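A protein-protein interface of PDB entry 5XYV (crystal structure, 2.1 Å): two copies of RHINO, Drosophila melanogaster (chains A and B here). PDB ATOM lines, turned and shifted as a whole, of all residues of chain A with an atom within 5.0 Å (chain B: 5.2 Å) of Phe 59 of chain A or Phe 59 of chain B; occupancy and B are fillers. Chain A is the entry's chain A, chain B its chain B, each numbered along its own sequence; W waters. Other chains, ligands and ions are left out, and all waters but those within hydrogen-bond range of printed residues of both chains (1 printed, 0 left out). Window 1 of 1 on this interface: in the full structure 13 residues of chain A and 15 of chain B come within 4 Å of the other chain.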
ATOM      1  N   CYS A  20       3.871   7.128   6.150  1.00  0.00           N
ATOM      2  CA  CYS A  20       2.853   6.171   5.777  1.00  0.00           C
ATOM      3  C   CYS A  20       2.336   6.472   4.378  1.00  0.00           C
ATOM      4  O   CYS A  20       2.470   7.583   3.874  1.00  0.00           O
ATOM      5  CB  CYS A  20       1.702   6.179   6.787  1.00  0.00           C
ATOM      6  SG  CYS A  20       0.629   7.647   6.719  1.00  0.00           S
ATOM      7  N   LEU A  27      -3.030   0.376   4.267  1.00  0.00           N
ATOM      8  CA  LEU A  27      -2.157   1.414   4.801  1.00  0.00           C
ATOM      9  C   LEU A  27      -0.784   0.814   5.156  1.00  0.00           C
ATOM     10  O   LEU A  27      -0.686  -0.158   5.896  1.00  0.00           O
ATOM     11  CB  LEU A  27      -2.808   2.094   6.019  1.00  0.00           C
ATOM     12  CG  LEU A  27      -2.041   3.244   6.685  1.00  0.00           C
ATOM     13  CD1 LEU A  27      -1.836   4.398   5.708  1.00  0.00           C
ATOM     14  CD2 LEU A  27      -2.749   3.749   7.932  1.00  0.00           C
ATOM     15  N   MET A  29       2.987   1.572   6.782  1.00  0.00           N
ATOM     16  CA  MET A  29       3.903   2.395   7.540  1.00  0.00           C
ATOM     17  C   MET A  29       5.335   2.134   7.082  1.00  0.00           C
ATOM     18  O   MET A  29       5.723   1.000   6.845  1.00  0.00           O
ATOM     19  CB  MET A  29       3.783   2.114   9.041  1.00  0.00           C
ATOM     20  CG  MET A  29       2.375   1.790   9.533  1.00  0.00           C
ATOM     21  SD  MET A  29       1.282   3.211   9.427  1.00  0.00           S
ATOM     22  CE  MET A  29       1.982   4.328  10.647  1.00  0.00           C
ATOM     23  N   ILE A  44       0.096  -1.846   8.138  1.00  0.00           N
ATOM     24  CA  ILE A  44      -0.310  -1.504   9.509  1.00  0.00           C
ATOM     25  C   ILE A  44      -0.815  -2.710  10.291  1.00  0.00           C
ATOM     26  O   ILE A  44      -0.540  -2.832  11.474  1.00  0.00           O
ATOM     27  CB  ILE A  44      -1.391  -0.396   9.536  1.00  0.00           C
ATOM     28  CG1 ILE A  44      -1.672   0.022  10.988  1.00  0.00           C
ATOM     29  CG2 ILE A  44      -2.673  -0.859   8.843  1.00  0.00           C
ATOM     30  CD1 ILE A  44      -2.076   1.444  11.139  1.00  0.00           C
ATOM     31  N   ILE A  55       1.977   3.925  16.821  1.00  0.00           N
ATOM     32  CA  ILE A  55       1.180   4.230  15.658  1.00  0.00           C
ATOM     33  C   ILE A  55       0.307   5.476  15.904  1.00  0.00           C
ATOM     34  O   ILE A  55       0.306   6.415  15.096  1.00  0.00           O
ATOM     35  CB  ILE A  55       0.328   3.029  15.264  1.00  0.00           C
ATOM     36  CG1 ILE A  55       1.257   1.882  14.822  1.00  0.00           C
ATOM     37  CG2 ILE A  55      -0.617   3.421  14.142  1.00  0.00           C
ATOM     38  CD1 ILE A  55       0.620   0.543  14.798  1.00  0.00           C
ATOM     39  N   ILE A  56      -0.408   5.489  17.028  1.00  0.00           N
ATOM     40  CA  ILE A  56      -1.298   6.602  17.355  1.00  0.00           C
ATOM     41  C   ILE A  56      -0.518   7.904  17.497  1.00  0.00           C
ATOM     42  O   ILE A  56      -0.943   8.946  17.009  1.00  0.00           O
ATOM     43  CB  ILE A  56      -2.087   6.316  18.628  1.00  0.00           C
ATOM     44  CG1 ILE A  56      -3.160   5.269  18.324  1.00  0.00           C
ATOM     45  CG2 ILE A  56      -2.744   7.606  19.161  1.00  0.00           C
ATOM     46  CD1 ILE A  56      -3.784   4.697  19.535  1.00  0.00           C
ATOM     47  N   LYS A  57       0.649   7.821  18.122  1.00  0.00           N
ATOM     48  CA  LYS A  57       1.530   8.966  18.266  1.00  0.00           C
ATOM     49  C   LYS A  57       1.960   9.498  16.887  1.00  0.00           C
ATOM     50  O   LYS A  57       1.985  10.702  16.663  1.00  0.00           O
ATOM     51  CB  LYS A  57       2.745   8.568  19.114  1.00  0.00           C
ATOM     52  CG  LYS A  57       3.414   9.679  19.872  1.00  0.00           C
ATOM     53  CD  LYS A  57       2.440  10.332  20.864  1.00  0.00           C
ATOM     54  CE  LYS A  57       3.135  11.455  21.657  1.00  0.00           C
ATOM     55  NZ  LYS A  57       2.216  12.553  22.176  1.00  0.00           N
ATOM     56  N   TYR A  58       2.282   8.603  15.954  1.00  0.00           N
ATOM     57  CA  TYR A  58       2.588   9.037  14.593  1.00  0.00           C
ATOM     58  C   TYR A  58       1.414   9.803  13.949  1.00  0.00           C
ATOM     59  O   TYR A  58       1.622  10.838  13.324  1.00  0.00           O
ATOM     60  CB  TYR A  58       2.967   7.850  13.695  1.00  0.00           C
ATOM     61  CG  TYR A  58       2.949   8.235  12.231  1.00  0.00           C
ATOM     62  CD1 TYR A  58       3.989   8.961  11.667  1.00  0.00           C
ATOM     63  CD2 TYR A  58       1.888   7.903  11.427  1.00  0.00           C
ATOM     64  CE1 TYR A  58       3.959   9.337  10.319  1.00  0.00           C
ATOM     65  CE2 TYR A  58       1.848   8.271  10.088  1.00  0.00           C
ATOM     66  CZ  TYR A  58       2.893   8.985   9.545  1.00  0.00           C
ATOM     67  OH  TYR A  58       2.836   9.357   8.226  1.00  0.00           O
ATOM     68  N   PHE A  59       0.195   9.276  14.061  1.00  0.00           N
ATOM     69  CA  PHE A  59      -0.968   9.972  13.513  1.00  0.00           C
ATOM     70  C   PHE A  59      -1.199  11.328  14.183  1.00  0.00           C
ATOM     71  O   PHE A  59      -1.615  12.268  13.527  1.00  0.00           O
ATOM     72  CB  PHE A  59      -2.231   9.142  13.658  1.00  0.00           C
ATOM     73  CG  PHE A  59      -2.345   8.032  12.669  1.00  0.00           C
ATOM     74  CD1 PHE A  59      -2.359   8.300  11.310  1.00  0.00           C
ATOM     75  CD2 PHE A  59      -2.495   6.728  13.092  1.00  0.00           C
ATOM     76  CE1 PHE A  59      -2.481   7.282  10.382  1.00  0.00           C
ATOM     77  CE2 PHE A  59      -2.611   5.689  12.170  1.00  0.00           C
ATOM     78  CZ  PHE A  59      -2.608   5.970  10.814  1.00  0.00           C
ATOM     79  N   GLU A  60      -0.955  11.407  15.490  1.00  0.00           N
ATOM     80  CA  GLU A  60      -1.050  12.672  16.224  1.00  0.00           C
ATOM     81  C   GLU A  60      -0.123  13.747  15.677  1.00  0.00           C
ATOM     82  O   GLU A  60      -0.418  14.933  15.761  1.00  0.00           O
ATOM     83  CB  GLU A  60      -0.725  12.461  17.696  1.00  0.00           C
ATOM     84  CG  GLU A  60      -1.865  11.909  18.515  1.00  0.00           C
ATOM     85  CD  GLU A  60      -1.489  11.807  19.977  1.00  0.00           C
ATOM     86  OE1 GLU A  60      -1.341  12.866  20.635  1.00  0.00           O
ATOM     87  OE2 GLU A  60      -1.317  10.670  20.461  1.00  0.00           O
ATOM     88  N   SER A  61       1.006  13.311  15.125  1.00  0.00           N
ATOM     89  CA  SER A  61       2.023  14.201  14.588  1.00  0.00           C
ATOM     90  C   SER A  61       1.613  14.795  13.250  1.00  0.00           C
ATOM     91  O   SER A  61       2.258  15.704  12.745  1.00  0.00           O
ATOM     92  CB  SER A  61       3.335  13.450  14.422  1.00  0.00           C
ATOM     93  OG  SER A  61       3.279  12.633  13.258  1.00  0.00           O
ATOM     94  N   LEU A  62       0.547  14.272  12.665  1.00  0.00           N
ATOM     95  CA  LEU A  62       0.092  14.786  11.382  1.00  0.00           C
ATOM     96  C   LEU A  62      -0.892  15.920  11.619  1.00  0.00           C
ATOM     97  O   LEU A  62      -1.499  16.012  12.691  1.00  0.00           O
ATOM     98  CB  LEU A  62      -0.576  13.694  10.537  1.00  0.00           C
ATOM     99  CG  LEU A  62       0.029  12.292  10.431  1.00  0.00           C
ATOM    100  CD1 LEU A  62      -0.491  11.554   9.206  1.00  0.00           C
ATOM    101  CD2 LEU A  62       1.523  12.293  10.473  1.00  0.00           C
ATOM    102  N   ILE A  64      -4.368  17.302  11.222  1.00  0.00           N
ATOM    103  CA  ILE A  64      -5.735  16.888  10.936  1.00  0.00           C
ATOM    104  C   ILE A  64      -6.595  18.123  10.732  1.00  0.00           C
ATOM    105  O   ILE A  64      -6.967  18.812  11.694  1.00  0.00           O
ATOM    106  CB  ILE A  64      -6.307  16.023  12.074  1.00  0.00           C
ATOM    107  CG1 ILE A  64      -5.288  14.948  12.460  1.00  0.00           C
ATOM    108  CG2 ILE A  64      -7.630  15.402  11.659  1.00  0.00           C
ATOM    109  CD1 ILE A  64      -5.703  14.090  13.612  1.00  0.00           C
ATOM    110  N   CYS B  20     -13.031  14.103  14.965  1.00  0.00           N
ATOM    111  CA  CYS B  20     -11.994  14.634  15.849  1.00  0.00           C
ATOM    112  C   CYS B  20     -11.646  16.080  15.521  1.00  0.00           C
ATOM    113  O   CYS B  20     -11.989  16.596  14.476  1.00  0.00           O
ATOM    114  CB  CYS B  20     -10.713  13.788  15.808  1.00  0.00           C
ATOM    115  SG  CYS B  20      -9.803  13.851  14.257  1.00  0.00           S
ATOM    116  N   LEU B  27      -5.395  16.750  20.732  1.00  0.00           N
ATOM    117  CA  LEU B  27      -6.344  16.112  19.840  1.00  0.00           C
ATOM    118  C   LEU B  27      -7.514  15.614  20.660  1.00  0.00           C
ATOM    119  O   LEU B  27      -7.340  14.848  21.614  1.00  0.00           O
ATOM    120  CB  LEU B  27      -5.701  14.949  19.063  1.00  0.00           C
ATOM    121  CG  LEU B  27      -6.530  14.233  17.989  1.00  0.00           C
ATOM    122  CD1 LEU B  27      -7.069  15.208  16.951  1.00  0.00           C
ATOM    123  CD2 LEU B  27      -5.747  13.072  17.313  1.00  0.00           C
ATOM    124  N   MET B  29     -11.329  13.681  20.571  1.00  0.00           N
ATOM    125  CA  MET B  29     -12.183  12.782  19.838  1.00  0.00           C
ATOM    126  C   MET B  29     -13.605  12.969  20.312  1.00  0.00           C
ATOM    127  O   MET B  29     -13.843  13.152  21.507  1.00  0.00           O
ATOM    128  CB  MET B  29     -11.733  11.331  20.036  1.00  0.00           C
ATOM    129  CG  MET B  29     -10.240  11.165  20.223  1.00  0.00           C
ATOM    130  SD  MET B  29      -9.372  11.224  18.647  1.00  0.00           S
ATOM    131  CE  MET B  29     -10.070   9.767  17.853  1.00  0.00           C
ATOM    132  N   ILE B  44      -7.502  12.564  23.503  1.00  0.00           N
ATOM    133  CA  ILE B  44      -7.064  11.285  22.942  1.00  0.00           C
ATOM    134  C   ILE B  44      -6.286  10.516  23.989  1.00  0.00           C
ATOM    135  O   ILE B  44      -6.290   9.281  23.988  1.00  0.00           O
ATOM    136  CB  ILE B  44      -6.194  11.438  21.646  1.00  0.00           C
ATOM    137  CG1 ILE B  44      -5.914  10.063  21.030  1.00  0.00           C
ATOM    138  CG2 ILE B  44      -4.865  12.147  21.912  1.00  0.00           C
ATOM    139  CD1 ILE B  44      -5.272  10.125  19.700  1.00  0.00           C
ATOM    140  N   ILE B  55      -9.217   3.276  17.877  1.00  0.00           N
ATOM    141  CA  ILE B  55      -8.685   4.577  17.502  1.00  0.00           C
ATOM    142  C   ILE B  55      -7.861   4.483  16.214  1.00  0.00           C
ATOM    143  O   ILE B  55      -7.978   5.336  15.341  1.00  0.00           O
ATOM    144  CB  ILE B  55      -7.810   5.174  18.640  1.00  0.00           C
ATOM    145  CG1 ILE B  55      -8.669   5.404  19.883  1.00  0.00           C
ATOM    146  CG2 ILE B  55      -7.137   6.479  18.200  1.00  0.00           C
ATOM    147  CD1 ILE B  55      -7.898   5.774  21.120  1.00  0.00           C
ATOM    148  N   ILE B  56      -7.030   3.443  16.111  1.00  0.00           N
ATOM    149  CA  ILE B  56      -6.241   3.195  14.917  1.00  0.00           C
ATOM    150  C   ILE B  56      -7.152   2.922  13.717  1.00  0.00           C
ATOM    151  O   ILE B  56      -6.892   3.406  12.607  1.00  0.00           O
ATOM    152  CB  ILE B  56      -5.270   2.016  15.133  1.00  0.00           C
ATOM    153  CG1 ILE B  56      -4.157   2.424  16.095  1.00  0.00           C
ATOM    154  CG2 ILE B  56      -4.669   1.538  13.827  1.00  0.00           C
ATOM    155  CD1 ILE B  56      -3.299   1.268  16.548  1.00  0.00           C
ATOM    156  N   LYS B  57      -8.238   2.187  13.938  1.00  0.00           N
ATOM    157  CA  LYS B  57      -9.149   1.896  12.837  1.00  0.00           C
ATOM    158  C   LYS B  57      -9.870   3.152  12.374  1.00  0.00           C
ATOM    159  O   LYS B  57     -10.157   3.298  11.193  1.00  0.00           O
ATOM    160  CB  LYS B  57     -10.159   0.806  13.218  1.00  0.00           C
ATOM    161  CG  LYS B  57     -10.379  -0.205  12.088  1.00  0.00           C
ATOM    162  CD  LYS B  57     -11.602  -1.105  12.297  1.00  0.00           C
ATOM    163  CE  LYS B  57     -11.619  -1.743  13.687  1.00  0.00           C
ATOM    164  NZ  LYS B  57     -10.453  -2.650  13.936  1.00  0.00           N
ATOM    165  N   TYR B  58     -10.160   4.056  13.303  1.00  0.00           N
ATOM    166  CA  TYR B  58     -10.751   5.340  12.943  1.00  0.00           C
ATOM    167  C   TYR B  58      -9.806   6.145  12.069  1.00  0.00           C
ATOM    168  O   TYR B  58     -10.231   6.738  11.091  1.00  0.00           O
ATOM    169  CB  TYR B  58     -11.128   6.160  14.184  1.00  0.00           C
ATOM    170  CG  TYR B  58     -11.479   7.595  13.830  1.00  0.00           C
ATOM    171  CD1 TYR B  58     -12.722   7.916  13.315  1.00  0.00           C
ATOM    172  CD2 TYR B  58     -10.557   8.621  13.997  1.00  0.00           C
ATOM    173  CE1 TYR B  58     -13.042   9.217  12.967  1.00  0.00           C
ATOM    174  CE2 TYR B  58     -10.861   9.918  13.652  1.00  0.00           C
ATOM    175  CZ  TYR B  58     -12.110  10.214  13.144  1.00  0.00           C
ATOM    176  OH  TYR B  58     -12.424  11.512  12.812  1.00  0.00           O
ATOM    177  N   PHE B  59      -8.535   6.195  12.446  1.00  0.00           N
ATOM    178  CA  PHE B  59      -7.555   6.901  11.628  1.00  0.00           C
ATOM    179  C   PHE B  59      -7.410   6.258  10.236  1.00  0.00           C
ATOM    180  O   PHE B  59      -7.255   6.962   9.246  1.00  0.00           O
ATOM    181  CB  PHE B  59      -6.198   6.961  12.326  1.00  0.00           C
ATOM    182  CG  PHE B  59      -6.125   7.996  13.399  1.00  0.00           C
ATOM    183  CD1 PHE B  59      -6.381   9.335  13.103  1.00  0.00           C
ATOM    184  CD2 PHE B  59      -5.783   7.649  14.700  1.00  0.00           C
ATOM    185  CE1 PHE B  59      -6.321  10.312  14.094  1.00  0.00           C
ATOM    186  CE2 PHE B  59      -5.706   8.621  15.705  1.00  0.00           C
ATOM    187  CZ  PHE B  59      -5.977   9.953  15.398  1.00  0.00           C
ATOM    188  N   GLU B  60      -7.479   4.930  10.171  1.00  0.00           N
ATOM    189  CA  GLU B  60      -7.408   4.217   8.894  1.00  0.00           C
ATOM    190  C   GLU B  60      -8.561   4.606   7.970  1.00  0.00           C
ATOM    191  O   GLU B  60      -8.400   4.608   6.758  1.00  0.00           O
ATOM    192  CB  GLU B  60      -7.415   2.694   9.108  1.00  0.00           C
ATOM    193  CG  GLU B  60      -6.097   2.086   9.547  1.00  0.00           C
ATOM    194  CD  GLU B  60      -6.199   0.571   9.761  1.00  0.00           C
ATOM    195  OE1 GLU B  60      -6.364  -0.165   8.757  1.00  0.00           O
ATOM    196  OE2 GLU B  60      -6.119   0.110  10.929  1.00  0.00           O
ATOM    197  N   SER B  61      -9.716   4.940   8.545  1.00  0.00           N
ATOM    198  CA  SER B  61     -10.912   5.244   7.758  1.00  0.00           C
ATOM    199  C   SER B  61     -10.812   6.626   7.109  1.00  0.00           C
ATOM    200  O   SER B  61     -11.507   6.918   6.132  1.00  0.00           O
ATOM    201  CB  SER B  61     -12.173   5.182   8.629  1.00  0.00           C
ATOM    202  OG  SER B  61     -12.221   6.268   9.546  1.00  0.00           O
ATOM    203  N   LEU B  62      -9.963   7.483   7.669  1.00  0.00           N
ATOM    204  CA  LEU B  62      -9.794   8.836   7.142  1.00  0.00           C
ATOM    205  C   LEU B  62      -8.976   8.802   5.859  1.00  0.00           C
ATOM    206  O   LEU B  62      -8.244   7.841   5.621  1.00  0.00           O
ATOM    207  CB  LEU B  62      -9.124   9.726   8.188  1.00  0.00           C
ATOM    208  CG  LEU B  62      -9.903   9.886   9.494  1.00  0.00           C
ATOM    209  CD1 LEU B  62      -9.143  10.764  10.480  1.00  0.00           C
ATOM    210  CD2 LEU B  62     -11.286  10.454   9.223  1.00  0.00           C
ATOM    211  N   ILE B  64      -5.843   9.878   4.056  1.00  0.00           N
ATOM    212  CA  ILE B  64      -4.508  10.407   4.318  1.00  0.00           C
ATOM    213  C   ILE B  64      -3.890  10.838   2.982  1.00  0.00           C
ATOM    214  O   ILE B  64      -3.640   9.994   2.111  1.00  0.00           O
ATOM    215  CB  ILE B  64      -3.631   9.357   5.014  1.00  0.00           C
ATOM    216  CG1 ILE B  64      -4.258   8.949   6.353  1.00  0.00           C
ATOM    217  CG2 ILE B  64      -2.222   9.886   5.222  1.00  0.00           C
ATOM    218  CD1 ILE B  64      -3.639   7.713   6.978  1.00  0.00           C
HETATM  219  O   HOH W   1      -5.039  -1.261   6.114  1.00  0.00           O
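Of the 13 printed residues of chain B, 7 touch a printed residue of chain A. Hydrophobic or aromatic side chains of chain B within 4 Å of the printed part of chain A: Leu 27, Ile 44, Ile 56, Phe 59 and Ile 64. Among the printed residues, 12 pairs touch across the chains.
Among the printed residues, merely in contact across the chains: Cys 20 of chain A with Ile 64 of chain B (3.9 Å), Leu 27 of chain A with Ile 64 of chain B (3.98 Å), Ile 44 of chain A with Ile 56 of chain B (3.7 Å), Ile 44 of chain A with Glu 60 of chain B (3.8 Å), Ile 56 of chain A with Ile 44 of chain B (3.6 Å), Ile 56 of chain A with Ile 56 of chain B (3.7 Å), Phe 59 of chain A with Phe 59 of chain B (3.8 Å), Phe 59 of chain A with Ile 64 of chain B (3.6 Å), Glu 60 of chain A with Ile 44 of chain B (3.8 Å), Ile 64 of chain A with Cys 20 of chain B (3.7 Å), Ile 64 of chain A with Leu 27 of chain B (3.8 Å) and Ile 64 of chain A with Phe 59 of chain B (3.9 Å).
Phe 59 of chain A touches just these residues of chain B: Phe 59 and Ile 64. Printed residues of chain A within 4 Å of Phe 59 of chain B: Phe 59 and Ile 64. Printed residues of chain B within 4 Å of Glu 60 of chain A: Ile 44. Of the printed residues of chain B, Ile 44 of chain A touches Ile 56 and Glu 60. Ser 61 of chain B touches none of the printed residues of chain A. Leu 62 of chain A touches none of the printed residues of chain B. The nearest residue of chain B that does not touch Phe 59 of chain A is Ile 56 of chain B (4.9 Å).
The side-chain sulfur (SG) of Cys 20 of chain A sits at hydrogen-bond distance from the side-chain hydroxyl (OH) of Tyr 58 of chain A, at 3.2 Å. N of Ile 44 of chain A sits at hydrogen-bond distance from O of Leu 27 of chain A, at 2.9 Å. NZ of Lys 57 of chain A is in salt-bridge range of OE1 of Glu 60 of chain A (3.9 Å). N of Cys 20 of chain B lies within hydrogen-bond range of OH of Tyr 58 of chain B. The backbone carbonyl oxygen (O) of Leu 27 of chain B sits at hydrogen-bond distance from the backbone NH (N) of Ile 44 of chain B, at 3.0 Å.
Cys 20 of chain A touches Ile 64 of chain B, and with the chains exchanged Ile 64 of chain A touches Cys 20 of chain B. Ile 44 of chain A touches Ile 56 of chain B, and with the chains exchanged Ile 56 of chain A touches Ile 44 of chain B. Ile 44 of chain A touches Glu 60 of chain B, and with the chains exchanged Glu 60 of chain A touches Ile 44 of chain B. Phe 59 of chain A touches its own counterpart, Phe 59 of chain B. 13 positions are printed for both chains. Of the 12 pairs that touch across the chains among the printed residues, 12 have their exchanged pair printed and touching as well.
Water W1 bridges OE1 of Glu 60 of chain B (3.2 Å) and N of Leu 27 of chain A (3.2 Å).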
